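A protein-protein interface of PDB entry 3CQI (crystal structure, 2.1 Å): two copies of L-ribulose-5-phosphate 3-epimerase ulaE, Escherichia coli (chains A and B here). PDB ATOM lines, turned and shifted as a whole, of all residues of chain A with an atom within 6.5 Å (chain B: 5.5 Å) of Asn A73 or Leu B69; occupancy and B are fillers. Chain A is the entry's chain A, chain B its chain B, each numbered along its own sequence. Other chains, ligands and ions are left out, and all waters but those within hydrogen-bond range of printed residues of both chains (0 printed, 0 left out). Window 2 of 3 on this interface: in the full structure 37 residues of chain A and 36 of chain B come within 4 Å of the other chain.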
ATOM      1  N   LEU A  33     -28.494  31.694  -6.583  1.00  0.00           N
ATOM      2  CA  LEU A  33     -29.421  30.756  -5.956  1.00  0.00           C
ATOM      3  C   LEU A  33     -30.613  31.503  -5.335  1.00  0.00           C
ATOM      4  O   LEU A  33     -31.759  31.089  -5.494  1.00  0.00           O
ATOM      5  CB  LEU A  33     -28.719  29.936  -4.869  1.00  0.00           C
ATOM      6  CG  LEU A  33     -29.164  28.493  -4.572  1.00  0.00           C
ATOM      7  CD1 LEU A  33     -28.907  28.167  -3.104  1.00  0.00           C
ATOM      8  CD2 LEU A  33     -30.606  28.167  -4.929  1.00  0.00           C
ATOM      9  N   ARG A  68     -19.283  29.459 -12.904  1.00  0.00           N
ATOM     10  CA  ARG A  68     -20.189  29.037 -13.990  1.00  0.00           C
ATOM     11  C   ARG A  68     -21.026  27.835 -13.585  1.00  0.00           C
ATOM     12  O   ARG A  68     -22.224  27.831 -13.786  1.00  0.00           O
ATOM     13  CB  ARG A  68     -19.401  28.735 -15.272  1.00  0.00           C
ATOM     14  CG  ARG A  68     -18.815  29.995 -15.905  1.00  0.00           C
ATOM     15  CD  ARG A  68     -17.644  29.723 -16.844  1.00  0.00           C
ATOM     16  NE  ARG A  68     -16.877  30.955 -17.005  1.00  0.00           N
ATOM     17  CZ  ARG A  68     -16.778  31.672 -18.122  1.00  0.00           C
ATOM     18  NH1 ARG A  68     -17.349  31.266 -19.253  1.00  0.00           N
ATOM     19  NH2 ARG A  68     -16.067  32.796 -18.113  1.00  0.00           N
ATOM     20  N   LEU A  69     -20.387  26.844 -12.969  1.00  0.00           N
ATOM     21  CA  LEU A  69     -21.050  25.604 -12.578  1.00  0.00           C
ATOM     22  C   LEU A  69     -21.969  25.781 -11.375  1.00  0.00           C
ATOM     23  O   LEU A  69     -22.905  25.006 -11.213  1.00  0.00           O
ATOM     24  CB  LEU A  69     -20.022  24.496 -12.330  1.00  0.00           C
ATOM     25  CG  LEU A  69     -19.217  24.021 -13.558  1.00  0.00           C
ATOM     26  CD1 LEU A  69     -18.121  23.033 -13.195  1.00  0.00           C
ATOM     27  CD2 LEU A  69     -20.133  23.422 -14.621  1.00  0.00           C
ATOM     28  N   ALA A  70     -21.691  26.782 -10.536  1.00  0.00           N
ATOM     29  CA  ALA A  70     -22.583  27.185  -9.441  1.00  0.00           C
ATOM     30  C   ALA A  70     -23.903  27.732  -9.975  1.00  0.00           C
ATOM     31  O   ALA A  70     -24.964  27.422  -9.435  1.00  0.00           O
ATOM     32  CB  ALA A  70     -21.923  28.229  -8.541  1.00  0.00           C
ATOM     33  N   LEU A  71     -23.834  28.567 -11.012  1.00  0.00           N
ATOM     34  CA  LEU A  71     -25.048  29.032 -11.668  1.00  0.00           C
ATOM     35  C   LEU A  71     -25.857  27.853 -12.205  1.00  0.00           C
ATOM     36  O   LEU A  71     -27.063  27.781 -11.963  1.00  0.00           O
ATOM     37  CB  LEU A  71     -24.755  30.060 -12.769  1.00  0.00           C
ATOM     38  CG  LEU A  71     -25.937  30.607 -13.588  1.00  0.00           C
ATOM     39  CD1 LEU A  71     -27.057  31.209 -12.706  1.00  0.00           C
ATOM     40  CD2 LEU A  71     -25.479  31.640 -14.619  1.00  0.00           C
ATOM     41  N   VAL A  72     -25.199  26.930 -12.908  1.00  0.00           N
ATOM     42  CA  VAL A  72     -25.890  25.751 -13.464  1.00  0.00           C
ATOM     43  C   VAL A  72     -26.591  24.980 -12.335  1.00  0.00           C
ATOM     44  O   VAL A  72     -27.770  24.623 -12.455  1.00  0.00           O
ATOM     45  CB  VAL A  72     -24.937  24.819 -14.275  1.00  0.00           C
ATOM     46  CG1 VAL A  72     -25.655  23.532 -14.701  1.00  0.00           C
ATOM     47  CG2 VAL A  72     -24.391  25.530 -15.508  1.00  0.00           C
ATOM     48  N   ASN A  73     -25.864  24.765 -11.232  1.00  0.00           N
ATOM     49  CA  ASN A  73     -26.410  24.131 -10.032  1.00  0.00           C
ATOM     50  C   ASN A  73     -27.648  24.813  -9.477  1.00  0.00           C
ATOM     51  O   ASN A  73     -28.627  24.152  -9.167  1.00  0.00           O
ATOM     52  CB  ASN A  73     -25.352  24.080  -8.929  1.00  0.00           C
ATOM     53  CG  ASN A  73     -24.731  22.716  -8.773  1.00  0.00           C
ATOM     54  OD1 ASN A  73     -25.064  21.980  -7.843  1.00  0.00           O
ATOM     55  ND2 ASN A  73     -23.799  22.372  -9.672  1.00  0.00           N
ATOM     56  N   ALA A  74     -27.591  26.137  -9.331  1.00  0.00           N
ATOM     57  CA  ALA A  74     -28.734  26.903  -8.856  1.00  0.00           C
ATOM     58  C   ALA A  74     -29.961  26.734  -9.768  1.00  0.00           C
ATOM     59  O   ALA A  74     -31.083  26.600  -9.286  1.00  0.00           O
ATOM     60  CB  ALA A  74     -28.357  28.364  -8.721  1.00  0.00           C
ATOM     61  N   ILE A  75     -29.733  26.743 -11.078  1.00  0.00           N
ATOM     62  CA  ILE A  75     -30.799  26.577 -12.080  1.00  0.00           C
ATOM     63  C   ILE A  75     -31.437  25.187 -11.975  1.00  0.00           C
ATOM     64  O   ILE A  75     -32.658  25.047 -11.915  1.00  0.00           O
ATOM     65  CB  ILE A  75     -30.250  26.798 -13.511  1.00  0.00           C
ATOM     66  CG1 ILE A  75     -29.909  28.276 -13.722  1.00  0.00           C
ATOM     67  CG2 ILE A  75     -31.230  26.253 -14.568  1.00  0.00           C
ATOM     68  CD1 ILE A  75     -28.958  28.536 -14.882  1.00  0.00           C
ATOM     69  N   VAL A  76     -30.596  24.162 -11.930  1.00  0.00           N
ATOM     70  CA  VAL A  76     -31.075  22.776 -11.867  1.00  0.00           C
ATOM     71  C   VAL A  76     -31.822  22.520 -10.546  1.00  0.00           C
ATOM     72  O   VAL A  76     -32.827  21.823 -10.520  1.00  0.00           O
ATOM     73  CB  VAL A  76     -29.909  21.774 -12.128  1.00  0.00           C
ATOM     74  CG1 VAL A  76     -30.225  20.380 -11.588  1.00  0.00           C
ATOM     75  CG2 VAL A  76     -29.596  21.704 -13.625  1.00  0.00           C
ATOM     76  N   GLU A  77     -31.344  23.125  -9.462  1.00  0.00           N
ATOM     77  CA  GLU A  77     -31.925  22.943  -8.131  1.00  0.00           C
ATOM     78  C   GLU A  77     -33.274  23.664  -7.919  1.00  0.00           C
ATOM     79  O   GLU A  77     -34.190  23.104  -7.303  1.00  0.00           O
ATOM     80  CB  GLU A  77     -30.886  23.342  -7.072  1.00  0.00           C
ATOM     81  CG  GLU A  77     -31.379  24.203  -5.917  1.00  0.00           C
ATOM     82  CD  GLU A  77     -30.420  24.210  -4.747  1.00  0.00           C
ATOM     83  OE1 GLU A  77     -29.216  24.554  -4.921  1.00  0.00           O
ATOM     84  OE2 GLU A  77     -30.880  23.863  -3.641  1.00  0.00           O
ATOM     85  N   THR A  78     -33.384  24.898  -8.418  1.00  0.00           N
ATOM     86  CA  THR A  78     -34.615  25.687  -8.276  1.00  0.00           C
ATOM     87  C   THR A  78     -35.646  25.377  -9.348  1.00  0.00           C
ATOM     88  O   THR A  78     -36.843  25.597  -9.131  1.00  0.00           O
ATOM     89  CB  THR A  78     -34.351  27.214  -8.315  1.00  0.00           C
ATOM     90  OG1 THR A  78     -33.699  27.568  -9.547  1.00  0.00           O
ATOM     91  CG2 THR A  78     -33.495  27.641  -7.138  1.00  0.00           C
ATOM     92  N   SER B  64     -30.902  11.447 -12.985  1.00  0.00           N
ATOM     93  CA  SER B  64     -31.141  12.303 -11.824  1.00  0.00           C
ATOM     94  C   SER B  64     -30.536  13.684 -12.065  1.00  0.00           C
ATOM     95  O   SER B  64     -29.776  13.869 -13.020  1.00  0.00           O
ATOM     96  CB  SER B  64     -30.520  11.677 -10.571  1.00  0.00           C
ATOM     97  OG  SER B  64     -29.113  11.630 -10.695  1.00  0.00           O
ATOM     98  N   ARG B  65     -30.871  14.649 -11.202  1.00  0.00           N
ATOM     99  CA  ARG B  65     -30.270  15.983 -11.291  1.00  0.00           C
ATOM    100  C   ARG B  65     -28.734  15.901 -11.167  1.00  0.00           C
ATOM    101  O   ARG B  65     -28.010  16.540 -11.932  1.00  0.00           O
ATOM    102  CB  ARG B  65     -30.882  16.936 -10.255  1.00  0.00           C
ATOM    103  CG  ARG B  65     -32.348  17.344 -10.548  1.00  0.00           C
ATOM    104  CD  ARG B  65     -33.044  17.893  -9.296  1.00  0.00           C
ATOM    105  NE  ARG B  65     -34.247  18.660  -9.631  1.00  0.00           N
ATOM    106  CZ  ARG B  65     -34.855  19.519  -8.806  1.00  0.00           C
ATOM    107  NH1 ARG B  65     -34.374  19.733  -7.577  1.00  0.00           N
ATOM    108  NH2 ARG B  65     -35.940  20.181  -9.209  1.00  0.00           N
ATOM    109  N   GLU B  66     -28.262  15.069 -10.237  1.00  0.00           N
ATOM    110  CA  GLU B  66     -26.830  14.808 -10.014  1.00  0.00           C
ATOM    111  C   GLU B  66     -26.099  14.200 -11.209  1.00  0.00           C
ATOM    112  O   GLU B  66     -24.934  14.509 -11.438  1.00  0.00           O
ATOM    113  CB  GLU B  66     -26.614  13.901  -8.778  1.00  0.00           C
ATOM    114  CG  GLU B  66     -26.995  14.556  -7.451  1.00  0.00           C
ATOM    115  CD  GLU B  66     -26.850  13.628  -6.254  1.00  0.00           C
ATOM    116  OE1 GLU B  66     -26.542  12.431  -6.443  1.00  0.00           O
ATOM    117  OE2 GLU B  66     -27.046  14.101  -5.115  1.00  0.00           O
ATOM    118  N   GLN B  67     -26.766  13.323 -11.952  1.00  0.00           N
ATOM    119  CA  GLN B  67     -26.138  12.703 -13.120  1.00  0.00           C
ATOM    120  C   GLN B  67     -25.956  13.725 -14.241  1.00  0.00           C
ATOM    121  O   GLN B  67     -24.920  13.756 -14.908  1.00  0.00           O
ATOM    122  CB  GLN B  67     -26.948  11.508 -13.608  1.00  0.00           C
ATOM    123  CG  GLN B  67     -26.779  10.275 -12.745  1.00  0.00           C
ATOM    124  CD  GLN B  67     -27.645   9.128 -13.212  1.00  0.00           C
ATOM    125  OE1 GLN B  67     -27.152   8.166 -13.801  1.00  0.00           O
ATOM    126  NE2 GLN B  67     -28.946   9.232 -12.972  1.00  0.00           N
ATOM    127  N   ARG B  68     -26.972  14.570 -14.411  1.00  0.00           N
ATOM    128  CA  ARG B  68     -26.971  15.648 -15.397  1.00  0.00           C
ATOM    129  C   ARG B  68     -25.873  16.669 -15.072  1.00  0.00           C
ATOM    130  O   ARG B  68     -25.088  17.062 -15.941  1.00  0.00           O
ATOM    131  CB  ARG B  68     -28.357  16.307 -15.413  1.00  0.00           C
ATOM    132  CG  ARG B  68     -29.411  15.504 -16.195  1.00  0.00           C
ATOM    133  CD  ARG B  68     -30.766  15.471 -15.507  1.00  0.00           C
ATOM    134  NE  ARG B  68     -31.783  15.964 -16.402  1.00  0.00           N
ATOM    135  CZ  ARG B  68     -32.791  15.275 -16.935  1.00  0.00           C
ATOM    136  NH1 ARG B  68     -33.022  13.990 -16.656  1.00  0.00           N
ATOM    137  NH2 ARG B  68     -33.593  15.925 -17.747  1.00  0.00           N
ATOM    138  N   LEU B  69     -25.812  17.075 -13.808  1.00  0.00           N
ATOM    139  CA  LEU B  69     -24.775  17.990 -13.336  1.00  0.00           C
ATOM    140  C   LEU B  69     -23.365  17.423 -13.509  1.00  0.00           C
ATOM    141  O   LEU B  69     -22.448  18.170 -13.824  1.00  0.00           O
ATOM    142  CB  LEU B  69     -25.029  18.415 -11.885  1.00  0.00           C
ATOM    143  CG  LEU B  69     -26.235  19.349 -11.693  1.00  0.00           C
ATOM    144  CD1 LEU B  69     -26.562  19.561 -10.200  1.00  0.00           C
ATOM    145  CD2 LEU B  69     -26.048  20.686 -12.419  1.00  0.00           C
ATOM    146  N   ALA B  70     -23.212  16.108 -13.319  1.00  0.00           N
ATOM    147  CA  ALA B  70     -21.935  15.412 -13.551  1.00  0.00           C
ATOM    148  C   ALA B  70     -21.442  15.515 -14.995  1.00  0.00           C
ATOM    149  O   ALA B  70     -20.243  15.678 -15.222  1.00  0.00           O
ATOM    150  CB  ALA B  70     -22.031  13.963 -13.144  1.00  0.00           C
ATOM    151  N   LEU B  71     -22.359  15.411 -15.966  1.00  0.00           N
ATOM    152  CA  LEU B  71     -22.014  15.574 -17.377  1.00  0.00           C
ATOM    153  C   LEU B  71     -21.563  17.005 -17.684  1.00  0.00           C
ATOM    154  O   LEU B  71     -20.523  17.213 -18.313  1.00  0.00           O
ATOM    155  CB  LEU B  71     -23.191  15.161 -18.285  1.00  0.00           C
ATOM    156  CG  LEU B  71     -22.979  15.296 -19.801  1.00  0.00           C
ATOM    157  CD1 LEU B  71     -21.687  14.575 -20.270  1.00  0.00           C
ATOM    158  CD2 LEU B  71     -24.217  14.821 -20.602  1.00  0.00           C
ATOM    159  N   VAL B  72     -22.341  17.989 -17.232  1.00  0.00           N
ATOM    160  CA  VAL B  72     -21.945  19.404 -17.342  1.00  0.00           C
ATOM    161  C   VAL B  72     -20.547  19.686 -16.756  1.00  0.00           C
ATOM    162  O   VAL B  72     -19.715  20.340 -17.395  1.00  0.00           O
ATOM    163  CB  VAL B  72     -22.999  20.327 -16.701  1.00  0.00           C
ATOM    164  CG1 VAL B  72     -22.557  21.794 -16.759  1.00  0.00           C
ATOM    165  CG2 VAL B  72     -24.352  20.145 -17.407  1.00  0.00           C
ATOM    166  N   ASN B  73     -20.302  19.179 -15.548  1.00  0.00           N
ATOM    167  CA  ASN B  73     -18.996  19.288 -14.895  1.00  0.00           C
ATOM    168  C   ASN B  73     -17.863  18.801 -15.792  1.00  0.00           C
ATOM    169  O   ASN B  73     -16.871  19.503 -15.976  1.00  0.00           O
ATOM    170  CB  ASN B  73     -18.983  18.482 -13.586  1.00  0.00           C
ATOM    171  CG  ASN B  73     -19.782  19.147 -12.472  1.00  0.00           C
ATOM    172  OD1 ASN B  73     -20.341  20.228 -12.648  1.00  0.00           O
ATOM    173  ND2 ASN B  73     -19.843  18.488 -11.316  1.00  0.00           N
ATOM    174  N   ALA B  74     -18.028  17.598 -16.344  1.00  0.00           N
ATOM    175  CA  ALA B  74     -17.067  16.984 -17.258  1.00  0.00           C
ATOM    176  C   ALA B  74     -16.860  17.776 -18.552  1.00  0.00           C
ATOM    177  O   ALA B  74     -15.730  17.868 -19.050  1.00  0.00           O
ATOM    178  CB  ALA B  74     -17.482  15.542 -17.570  1.00  0.00           C
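The backbone carbonyl oxygen (O) of Glu A77 lies within hydrogen-bond range of the guanidinium group (NH1) of Arg B65.
Leu A69 touches Val B72, and with the chains exchanged Val A72 touches Leu B69.
Leu A69 touches Asn B73, and with the chains exchanged Asn A73 touches Leu B69.
Positions printed for both chains: 68, 69, 70, 71, 72, 73 and 74.
Of the 7 pairs that touch across the chains among the printed residues, 4 have their exchanged pair printed and touching as well.
O of Leu A69 sits at hydrogen-bond distance from ND2 of Asn A73 (3.2 Å).
O of Leu B69 lies close to OD1 of Asn B73, at 3.2 Å.
Val B72 touches Leu A69 (CG1 to CD2, 3.6 Å).
Leu A69 touches Asn B73.
Val A72 touches Leu B69.
Asn A73 touches Leu B69 (OD1 to CD1, 3.7 Å).
Val A76 touches Arg B65 (O to CZ, 3.5 Å).
CG2 of Val A76 touches CD2 of Leu B69, at 3.9 Å.
Of the 12 printed residues of chain A, 5 touch a printed residue of chain B.
Along chain A the printed residues that touch a printed residue of chain B span positions 69 to 77.
Of the 11 printed residues of chain B, 4 touch a printed residue of chain A.
Hydrophobic or aromatic side chains of chain B that line the printed part of chain A: Leu B69 and Val B72.
Among the printed residues, 7 pairs touch across the chains.
Of chain B, only Leu B69 comes within 4 Å of Asn A73.
Of the printed residues of chain A, Val B72 touches Leu A69 (3.6 Å).
Of the printed residues of chain B, Leu A69 touches Val B72 (3.6 Å) and Asn B73 (3.6 Å).
Printed residues of chain B within 4 Å of Val A72: Leu B69.
Of the printed residues of chain A, Arg B65 touches Val A76 and Glu A77.
The nearest residue of chain A that does not touch Leu B69 is Leu A69 (5.5 Å).
The nearest printed residue of chain B that does not touch Val A76 is Arg B68 (5.8 Å).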
